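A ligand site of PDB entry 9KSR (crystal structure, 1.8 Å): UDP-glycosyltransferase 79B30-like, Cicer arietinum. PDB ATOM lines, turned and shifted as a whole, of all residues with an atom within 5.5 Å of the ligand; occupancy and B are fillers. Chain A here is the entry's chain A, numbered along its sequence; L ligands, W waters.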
ATOM      1  N   MET A  13      -9.419  31.680  16.345  1.00  0.00           N
ATOM      2  CA  MET A  13     -10.874  31.817  16.324  1.00  0.00           C
ATOM      3  C   MET A  13     -11.550  31.080  17.470  1.00  0.00           C
ATOM      4  O   MET A  13     -12.582  31.558  17.957  1.00  0.00           O
ATOM      5  CB  MET A  13     -11.456  31.392  14.972  1.00  0.00           C
ATOM      6  CG  MET A  13     -10.728  31.989  13.774  1.00  0.00           C
ATOM      7  SD  MET A  13     -11.195  33.756  13.763  1.00  0.00           S
ATOM      8  CE  MET A  13     -12.979  33.684  13.674  1.00  0.00           C
ATOM      9  N   GLY A  14     -10.958  29.993  17.972  1.00  0.00           N
ATOM     10  CA  GLY A  14     -11.570  29.294  19.112  1.00  0.00           C
ATOM     11  C   GLY A  14     -11.478  30.044  20.426  1.00  0.00           C
ATOM     12  O   GLY A  14     -12.106  29.631  21.411  1.00  0.00           O
ATOM     13  N   ILE A  17     -14.005  33.792  19.331  1.00  0.00           N
ATOM     14  CA  ILE A  17     -15.460  33.587  19.249  1.00  0.00           C
ATOM     15  C   ILE A  17     -16.089  33.466  20.643  1.00  0.00           C
ATOM     16  O   ILE A  17     -17.058  34.192  20.919  1.00  0.00           O
ATOM     17  CB  ILE A  17     -15.785  32.373  18.365  1.00  0.00           C
ATOM     18  CG1 ILE A  17     -15.432  32.662  16.900  1.00  0.00           C
ATOM     19  CG2 ILE A  17     -17.250  31.981  18.544  1.00  0.00           C
ATOM     20  CD1 ILE A  17     -15.689  31.511  15.925  1.00  0.00           C
ATOM     21  N   TYR A 265     -22.258  15.074  10.310  1.00  0.00           N
ATOM     22  CA  TYR A 265     -21.408  16.250  10.157  1.00  0.00           C
ATOM     23  C   TYR A 265     -20.076  15.983  10.853  1.00  0.00           C
ATOM     24  O   TYR A 265     -20.048  15.568  12.018  1.00  0.00           O
ATOM     25  CB  TYR A 265     -22.083  17.486  10.779  1.00  0.00           C
ATOM     26  CG  TYR A 265     -21.209  18.723  10.821  1.00  0.00           C
ATOM     27  CD1 TYR A 265     -20.977  19.486   9.668  1.00  0.00           C
ATOM     28  CD2 TYR A 265     -20.612  19.132  12.018  1.00  0.00           C
ATOM     29  CE1 TYR A 265     -20.162  20.632   9.724  1.00  0.00           C
ATOM     30  CE2 TYR A 265     -19.800  20.261  12.074  1.00  0.00           C
ATOM     31  CZ  TYR A 265     -19.578  21.014  10.919  1.00  0.00           C
ATOM     32  OH  TYR A 265     -18.772  22.132  10.945  1.00  0.00           O
ATOM     33  N   LEU A 268     -13.071  19.258  12.282  1.00  0.00           N
ATOM     34  CA  LEU A 268     -11.965  19.202  13.232  1.00  0.00           C
ATOM     35  C   LEU A 268     -11.404  20.599  13.491  1.00  0.00           C
ATOM     36  O   LEU A 268     -10.199  20.791  13.608  1.00  0.00           O
ATOM     37  CB  LEU A 268     -10.871  18.249  12.740  1.00  0.00           C
ATOM     38  CG  LEU A 268     -11.311  16.842  12.268  1.00  0.00           C
ATOM     39  CD1 LEU A 268     -10.126  15.986  11.794  1.00  0.00           C
ATOM     40  CD2 LEU A 268     -12.138  16.110  13.333  1.00  0.00           C
ATOM     41  N   GLY A 269     -12.286  21.599  13.552  1.00  0.00           N
ATOM     42  CA  GLY A 269     -11.892  22.958  13.897  1.00  0.00           C
ATOM     43  C   GLY A 269     -11.154  23.629  12.736  1.00  0.00           C
ATOM     44  O   GLY A 269     -11.147  23.163  11.600  1.00  0.00           O
ATOM     45  N   SER A 270     -10.473  24.733  13.047  1.00  0.00           N
ATOM     46  CA  SER A 270      -9.850  25.527  11.996  1.00  0.00           C
ATOM     47  C   SER A 270      -8.343  25.602  12.110  1.00  0.00           C
ATOM     48  O   SER A 270      -7.731  26.406  11.399  1.00  0.00           O
ATOM     49  CB  SER A 270     -10.422  26.953  12.005  1.00  0.00           C
ATOM     50  OG  SER A 270     -10.007  27.609  13.198  1.00  0.00           O
ATOM     51  N   GLU A 271      -7.713  24.815  12.983  1.00  0.00           N
ATOM     52  CA  GLU A 271      -6.283  24.951  13.204  1.00  0.00           C
ATOM     53  C   GLU A 271      -5.474  23.780  12.691  1.00  0.00           C
ATOM     54  O   GLU A 271      -4.236  23.866  12.704  1.00  0.00           O
ATOM     55  CB  GLU A 271      -5.984  25.107  14.698  1.00  0.00           C
ATOM     56  CG  GLU A 271      -6.637  26.245  15.400  1.00  0.00           C
ATOM     57  CD  GLU A 271      -6.223  26.270  16.856  1.00  0.00           C
ATOM     58  OE1 GLU A 271      -6.381  25.224  17.516  1.00  0.00           O
ATOM     59  OE2 GLU A 271      -5.712  27.313  17.310  1.00  0.00           O
ATOM     60  N   LEU A 272      -6.112  22.684  12.299  1.00  0.00           N
ATOM     61  CA  LEU A 272      -5.408  21.413  12.158  1.00  0.00           C
ATOM     62  C   LEU A 272      -5.538  20.875  10.749  1.00  0.00           C
ATOM     63  O   LEU A 272      -6.545  21.079  10.068  1.00  0.00           O
ATOM     64  CB  LEU A 272      -5.967  20.339  13.099  1.00  0.00           C
ATOM     65  CG  LEU A 272      -6.606  20.582  14.453  1.00  0.00           C
ATOM     66  CD1 LEU A 272      -7.019  19.242  15.010  1.00  0.00           C
ATOM     67  CD2 LEU A 272      -5.752  21.363  15.477  1.00  0.00           C
ATOM     68  N   ILE A 296     -15.863  18.831   7.022  1.00  0.00           N
ATOM     69  CA  ILE A 296     -15.196  20.124   6.914  1.00  0.00           C
ATOM     70  C   ILE A 296     -13.755  19.914   7.345  1.00  0.00           C
ATOM     71  O   ILE A 296     -13.447  19.873   8.546  1.00  0.00           O
ATOM     72  CB  ILE A 296     -15.882  21.198   7.767  1.00  0.00           C
ATOM     73  CG1 ILE A 296     -17.393  21.216   7.461  1.00  0.00           C
ATOM     74  CG2 ILE A 296     -15.240  22.580   7.508  1.00  0.00           C
ATOM     75  CD1 ILE A 296     -17.710  21.510   5.991  1.00  0.00           C
ATOM     76  N   GLY A 327     -13.357  25.035   3.131  1.00  0.00           N
ATOM     77  CA  GLY A 327     -13.554  26.421   3.559  1.00  0.00           C
ATOM     78  C   GLY A 327     -14.222  26.563   4.930  1.00  0.00           C
ATOM     79  O   GLY A 327     -14.864  25.646   5.444  1.00  0.00           O
ATOM     80  N   TRP A 328     -14.065  27.755   5.510  1.00  0.00           N
ATOM     81  CA  TRP A 328     -14.782  28.135   6.736  1.00  0.00           C
ATOM     82  C   TRP A 328     -16.294  28.116   6.507  1.00  0.00           C
ATOM     83  O   TRP A 328     -16.781  28.740   5.563  1.00  0.00           O
ATOM     84  CB  TRP A 328     -14.334  29.519   7.180  1.00  0.00           C
ATOM     85  CG  TRP A 328     -15.012  30.044   8.419  1.00  0.00           C
ATOM     86  CD1 TRP A 328     -16.201  30.707   8.499  1.00  0.00           C
ATOM     87  CD2 TRP A 328     -14.524  29.917   9.754  1.00  0.00           C
ATOM     88  NE1 TRP A 328     -16.481  31.007   9.823  1.00  0.00           N
ATOM     89  CE2 TRP A 328     -15.461  30.536  10.609  1.00  0.00           C
ATOM     90  CE3 TRP A 328     -13.374  29.341  10.318  1.00  0.00           C
ATOM     91  CZ2 TRP A 328     -15.294  30.585  11.995  1.00  0.00           C
ATOM     92  CZ3 TRP A 328     -13.208  29.403  11.697  1.00  0.00           C
ATOM     93  CH2 TRP A 328     -14.164  30.025  12.507  1.00  0.00           C
ATOM     94  N   ILE A 329     -17.042  27.449   7.383  1.00  0.00           N
ATOM     95  CA  ILE A 329     -18.496  27.431   7.268  1.00  0.00           C
ATOM     96  C   ILE A 329     -19.117  27.865   8.590  1.00  0.00           C
ATOM     97  O   ILE A 329     -18.428  28.016   9.595  1.00  0.00           O
ATOM     98  CB  ILE A 329     -19.059  26.069   6.804  1.00  0.00           C
ATOM     99  CG1 ILE A 329     -18.381  24.873   7.478  1.00  0.00           C
ATOM    100  CG2 ILE A 329     -18.873  25.928   5.293  1.00  0.00           C
ATOM    101  CD1 ILE A 329     -18.523  24.811   8.970  1.00  0.00           C
ATOM    102  N   GLN A 330     -20.442  28.053   8.585  1.00  0.00           N
ATOM    103  CA  GLN A 330     -21.172  28.476   9.788  1.00  0.00           C
ATOM    104  C   GLN A 330     -21.537  27.245  10.615  1.00  0.00           C
ATOM    105  O   GLN A 330     -22.663  26.753  10.603  1.00  0.00           O
ATOM    106  CB  GLN A 330     -22.401  29.297   9.417  1.00  0.00           C
ATOM    107  CG  GLN A 330     -22.076  30.478   8.514  1.00  0.00           C
ATOM    108  CD  GLN A 330     -23.306  30.965   7.776  1.00  0.00           C
ATOM    109  OE1 GLN A 330     -23.628  30.450   6.702  1.00  0.00           O
ATOM    110  NE2 GLN A 330     -23.974  31.981   8.317  1.00  0.00           N
ATOM    111  N   GLN A 331     -20.541  26.743  11.355  1.00  0.00           N
ATOM    112  CA  GLN A 331     -20.698  25.469  12.048  1.00  0.00           C
ATOM    113  C   GLN A 331     -21.897  25.486  12.994  1.00  0.00           C
ATOM    114  O   GLN A 331     -22.704  24.547  13.020  1.00  0.00           O
ATOM    115  CB  GLN A 331     -19.437  25.122  12.834  1.00  0.00           C
ATOM    116  CG  GLN A 331     -19.652  23.909  13.714  1.00  0.00           C
ATOM    117  CD  GLN A 331     -18.361  23.281  14.173  1.00  0.00           C
ATOM    118  OE1 GLN A 331     -17.648  22.692  13.364  1.00  0.00           O
ATOM    119  NE2 GLN A 331     -18.065  23.385  15.481  1.00  0.00           N
ATOM    120  N   GLN A 332     -22.016  26.541  13.798  1.00  0.00           N
ATOM    121  CA  GLN A 332     -23.103  26.606  14.771  1.00  0.00           C
ATOM    122  C   GLN A 332     -24.444  26.483  14.077  1.00  0.00           C
ATOM    123  O   GLN A 332     -25.334  25.782  14.552  1.00  0.00           O
ATOM    124  CB  GLN A 332     -23.016  27.907  15.565  1.00  0.00           C
ATOM    125  CG  GLN A 332     -24.247  28.241  16.384  1.00  0.00           C
ATOM    126  CD  GLN A 332     -24.171  29.625  16.971  1.00  0.00           C
ATOM    127  OE1 GLN A 332     -23.088  30.213  17.072  1.00  0.00           O
ATOM    128  NE2 GLN A 332     -25.327  30.177  17.316  1.00  0.00           N
ATOM    129  N   HIS A 346     -13.507  16.869  16.745  1.00  0.00           N
ATOM    130  CA  HIS A 346     -12.151  16.802  17.296  1.00  0.00           C
ATOM    131  C   HIS A 346     -12.097  17.179  18.773  1.00  0.00           C
ATOM    132  O   HIS A 346     -11.009  17.182  19.366  1.00  0.00           O
ATOM    133  CB  HIS A 346     -11.195  17.695  16.476  1.00  0.00           C
ATOM    134  CG  HIS A 346     -11.295  19.158  16.802  1.00  0.00           C
ATOM    135  ND1 HIS A 346     -12.496  19.835  16.852  1.00  0.00           N
ATOM    136  CD2 HIS A 346     -10.330  20.074  17.036  1.00  0.00           C
ATOM    137  CE1 HIS A 346     -12.266  21.101  17.135  1.00  0.00           C
ATOM    138  NE2 HIS A 346     -10.956  21.273  17.250  1.00  0.00           N
ATOM    139  N   GLY A 348     -12.581  20.014  20.303  1.00  0.00           N
ATOM    140  CA  GLY A 348     -12.354  21.394  20.708  1.00  0.00           C
ATOM    141  C   GLY A 348     -13.466  21.878  21.627  1.00  0.00           C
ATOM    142  O   GLY A 348     -14.633  21.530  21.463  1.00  0.00           O
ATOM    143  N   ALA A 349     -13.089  22.691  22.619  1.00  0.00           N
ATOM    144  CA  ALA A 349     -14.043  23.091  23.640  1.00  0.00           C
ATOM    145  C   ALA A 349     -15.242  23.832  23.058  1.00  0.00           C
ATOM    146  O   ALA A 349     -16.355  23.737  23.614  1.00  0.00           O
ATOM    147  CB  ALA A 349     -13.341  23.975  24.677  1.00  0.00           C
ATOM    148  N   GLY A 350     -15.051  24.559  21.964  1.00  0.00           N
ATOM    149  CA  GLY A 350     -16.133  25.336  21.374  1.00  0.00           C
ATOM    150  C   GLY A 350     -17.109  24.429  20.655  1.00  0.00           C
ATOM    151  O   GLY A 350     -18.334  24.553  20.823  1.00  0.00           O
ATOM    152  N   SER A 351     -16.557  23.512  19.859  1.00  0.00           N
ATOM    153  CA  SER A 351     -17.341  22.491  19.168  1.00  0.00           C
ATOM    154  C   SER A 351     -18.098  21.606  20.153  1.00  0.00           C
ATOM    155  O   SER A 351     -19.249  21.235  19.891  1.00  0.00           O
ATOM    156  CB  SER A 351     -16.442  21.639  18.292  1.00  0.00           C
ATOM    157  OG  SER A 351     -15.938  22.404  17.191  1.00  0.00           O
ATOM    158  N   ILE A 352     -17.468  21.255  21.274  1.00  0.00           N
ATOM    159  CA  ILE A 352     -18.157  20.476  22.311  1.00  0.00           C
ATOM    160  C   ILE A 352     -19.419  21.191  22.774  1.00  0.00           C
ATOM    161  O   ILE A 352     -20.503  20.604  22.830  1.00  0.00           O
ATOM    162  CB  ILE A 352     -17.220  20.209  23.503  1.00  0.00           C
ATOM    163  CG1 ILE A 352     -16.111  19.215  23.161  1.00  0.00           C
ATOM    164  CG2 ILE A 352     -18.021  19.635  24.672  1.00  0.00           C
ATOM    165  CD1 ILE A 352     -16.606  17.860  22.761  1.00  0.00           C
ATOM    166  N   GLU A 354     -21.131  23.480  21.263  1.00  0.00           N
ATOM    167  CA  GLU A 354     -22.091  23.601  20.166  1.00  0.00           C
ATOM    168  C   GLU A 354     -22.794  22.272  19.886  1.00  0.00           C
ATOM    169  O   GLU A 354     -23.976  22.264  19.503  1.00  0.00           O
ATOM    170  CB  GLU A 354     -21.371  24.142  18.931  1.00  0.00           C
ATOM    171  CG  GLU A 354     -20.946  25.594  19.145  1.00  0.00           C
ATOM    172  CD  GLU A 354     -19.829  26.077  18.224  1.00  0.00           C
ATOM    173  OE1 GLU A 354     -19.431  25.360  17.286  1.00  0.00           O
ATOM    174  OE2 GLU A 354     -19.357  27.213  18.441  1.00  0.00           O
ATOM    175  N   TYR A 372      -8.215  18.580  23.862  1.00  0.00           N
ATOM    176  CA  TYR A 372      -9.112  17.710  23.103  1.00  0.00           C
ATOM    177  C   TYR A 372      -9.221  16.333  23.721  1.00  0.00           C
ATOM    178  O   TYR A 372     -10.311  15.740  23.783  1.00  0.00           O
ATOM    179  CB  TYR A 372      -8.624  17.560  21.661  1.00  0.00           C
ATOM    180  CG  TYR A 372      -8.394  18.844  20.884  1.00  0.00           C
ATOM    181  CD1 TYR A 372      -8.953  20.047  21.284  1.00  0.00           C
ATOM    182  CD2 TYR A 372      -7.574  18.844  19.746  1.00  0.00           C
ATOM    183  CE1 TYR A 372      -8.735  21.221  20.547  1.00  0.00           C
ATOM    184  CE2 TYR A 372      -7.336  20.026  19.033  1.00  0.00           C
ATOM    185  CZ  TYR A 372      -7.926  21.198  19.442  1.00  0.00           C
ATOM    186  OH  TYR A 372      -7.689  22.351  18.736  1.00  0.00           O
HETATM  187  N1  LIG L   1     -15.853  27.145  13.342  1.00  0.00           N
HETATM  188  C1  LIG L   1     -16.693  27.626  12.363  1.00  0.00           C
HETATM  189  N2  LIG L   1     -16.399  27.200  11.089  1.00  0.00           N
HETATM  190  C2  LIG L   1     -15.347  26.390  10.708  1.00  0.00           C
HETATM  191  C3  LIG L   1     -14.508  25.947  11.779  1.00  0.00           C
HETATM  192  C4  LIG L   1     -14.781  26.335  13.041  1.00  0.00           C
HETATM  193  O1  LIG L   1     -17.646  28.351  12.606  1.00  0.00           O
HETATM  194  O2  LIG L   1     -15.199  26.110   9.518  1.00  0.00           O
HETATM  195  C5  LIG L   1     -16.092  27.624  14.709  1.00  0.00           C
HETATM  196  C6  LIG L   1     -16.750  26.605  15.640  1.00  0.00           C
HETATM  197  O3  LIG L   1     -18.147  26.690  15.518  1.00  0.00           O
HETATM  198  C7  LIG L   1     -16.228  27.084  17.000  1.00  0.00           C
HETATM  199  C8  LIG L   1     -14.801  27.521  16.654  1.00  0.00           C
HETATM  200  O4  LIG L   1     -14.835  27.920  15.267  1.00  0.00           O
HETATM  201  O5  LIG L   1     -16.976  28.163  17.554  1.00  0.00           O
HETATM  202  C9  LIG L   1     -13.773  26.432  16.772  1.00  0.00           C
HETATM  203  O6  LIG L   1     -13.532  26.267  18.156  1.00  0.00           O
HETATM  204  P1  LIG L   1     -13.069  24.847  18.726  1.00  0.00           P
HETATM  205  O7  LIG L   1     -12.566  25.119  20.102  1.00  0.00           O
HETATM  206  O8  LIG L   1     -14.157  23.836  18.541  1.00  0.00           O
HETATM  207  O9  LIG L   1     -11.892  24.392  17.715  1.00  0.00           O
HETATM  208  P2  LIG L   1     -10.551  24.978  17.027  1.00  0.00           P
HETATM  209  O10 LIG L   1     -10.943  25.467  15.650  1.00  0.00           O
HETATM  210  O11 LIG L   1     -10.002  26.079  17.920  1.00  0.00           O
HETATM  211  O12 LIG L   1      -9.629  23.774  16.989  1.00  0.00           O
HETATM  212  O   HOH W   1      -8.046  27.163  19.606  1.00  0.00           O
HETATM  213  O   HOH W   2     -16.086  28.744  20.160  1.00  0.00           O
HETATM  214  O   HOH W   3      -8.596  22.760  14.773  1.00  0.00           O
HETATM  215  O   HOH W   4      -8.888  28.180  17.132  1.00  0.00           O
HETATM  216  O   HOH W   5     -13.515  27.516  21.447  1.00  0.00           O
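The side-chain amide nitrogen of Gln 331 lies within hydrogen-bond range of the side-chain hydroxyl of Ser 351 (2.9 Å).
The backbone NH of Gly 348 lies close to a ring nitrogen (ND1) of His 346, 3.5 Å away.
OH of Tyr 265 is in hydrogen-bond range of OE1 of Gln 331, at 2.7 Å.
The side-chain amide nitrogen of Gln 331 sits at hydrogen-bond distance from the side-chain carboxylate of Glu 354, 3.0 Å away.
OH of Tyr 372 is in hydrogen-bond range of OE1 of Glu 271 (3.4 Å).
NE2 of His 346 lies within hydrogen-bond range of O12 of the ligand (2.8 Å).
An oxygen (O10) of the ligand sits at hydrogen-bond distance from the backbone NH of Ser 270, 2.7 Å away.
The side-chain hydroxyl of Ser 270 is in hydrogen-bond range of an oxygen (O10) of the ligand.
An oxygen (O2) of the ligand lies within hydrogen-bond range of the backbone NH (N) of Ile 329, 3.1 Å away.
The side-chain amide nitrogen (NE2) of Gln 331 lies within hydrogen-bond range of an oxygen (O3) of the ligand, at 3.3 Å.
An oxygen (O7) of the ligand sits at hydrogen-bond distance from the backbone NH of Gly 350, 3.2 Å away.
The backbone NH (N) of Ser 351 is in hydrogen-bond range of an oxygen (O8) of the ligand, 2.8 Å away.
O of Ile 329 sits at hydrogen-bond distance from N2 of the ligand.
OH of Tyr 372 sits at hydrogen-bond distance from O12 of the ligand, at 3.0 Å.
The side-chain hydroxyl (OG) of Ser 351 is in hydrogen-bond range of an oxygen (O8) of the ligand (2.7 Å).
An oxygen (O3) of the ligand is in hydrogen-bond range of the side-chain carboxylate of Glu 354, 2.6 Å away.
Gly 14 touches the ligand (CA to O6, 3.7 Å).
Ile 17 touches the ligand (CD1 to O4, 3.7 Å).
CA of Gly 269 touches O10 of the ligand, at 3.2 Å.
Glu 271 touches the ligand.
Trp 328 touches the ligand (CZ2 to C1, 3.3 Å).
Gly 348 touches the ligand.
N of Ala 349 touches O7 of the ligand (3.5 Å).
Within 4 Å of the ligand: Gly 14, Ile 17, Gly 269, Ser 270, Glu 271, Trp 328, Ile 329, Gln 331, His 346, Gly 348, Ala 349, Gly 350, Ser 351, Glu 354 and Tyr 372.
Water W4 lies within hydrogen-bond range of O11 of the ligand (2.5 Å), N of Gly 14 (2.9 Å) and OE2 of Glu 271 (3.3 Å).
Water W3 lies within hydrogen-bond range of O12 of the ligand, O of Leu 268, N of Glu 271 and N of Ser 270.
Water W1 lies within hydrogen-bond range of O11 of the ligand (2.8 Å) and OE2 of Glu 271 (3.3 Å).
Water W5 lies within hydrogen-bond range of the backbone carbonyl oxygen (O) of Gly 14, an oxygen (O7) of the ligand and the backbone NH (N) of Gly 350.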
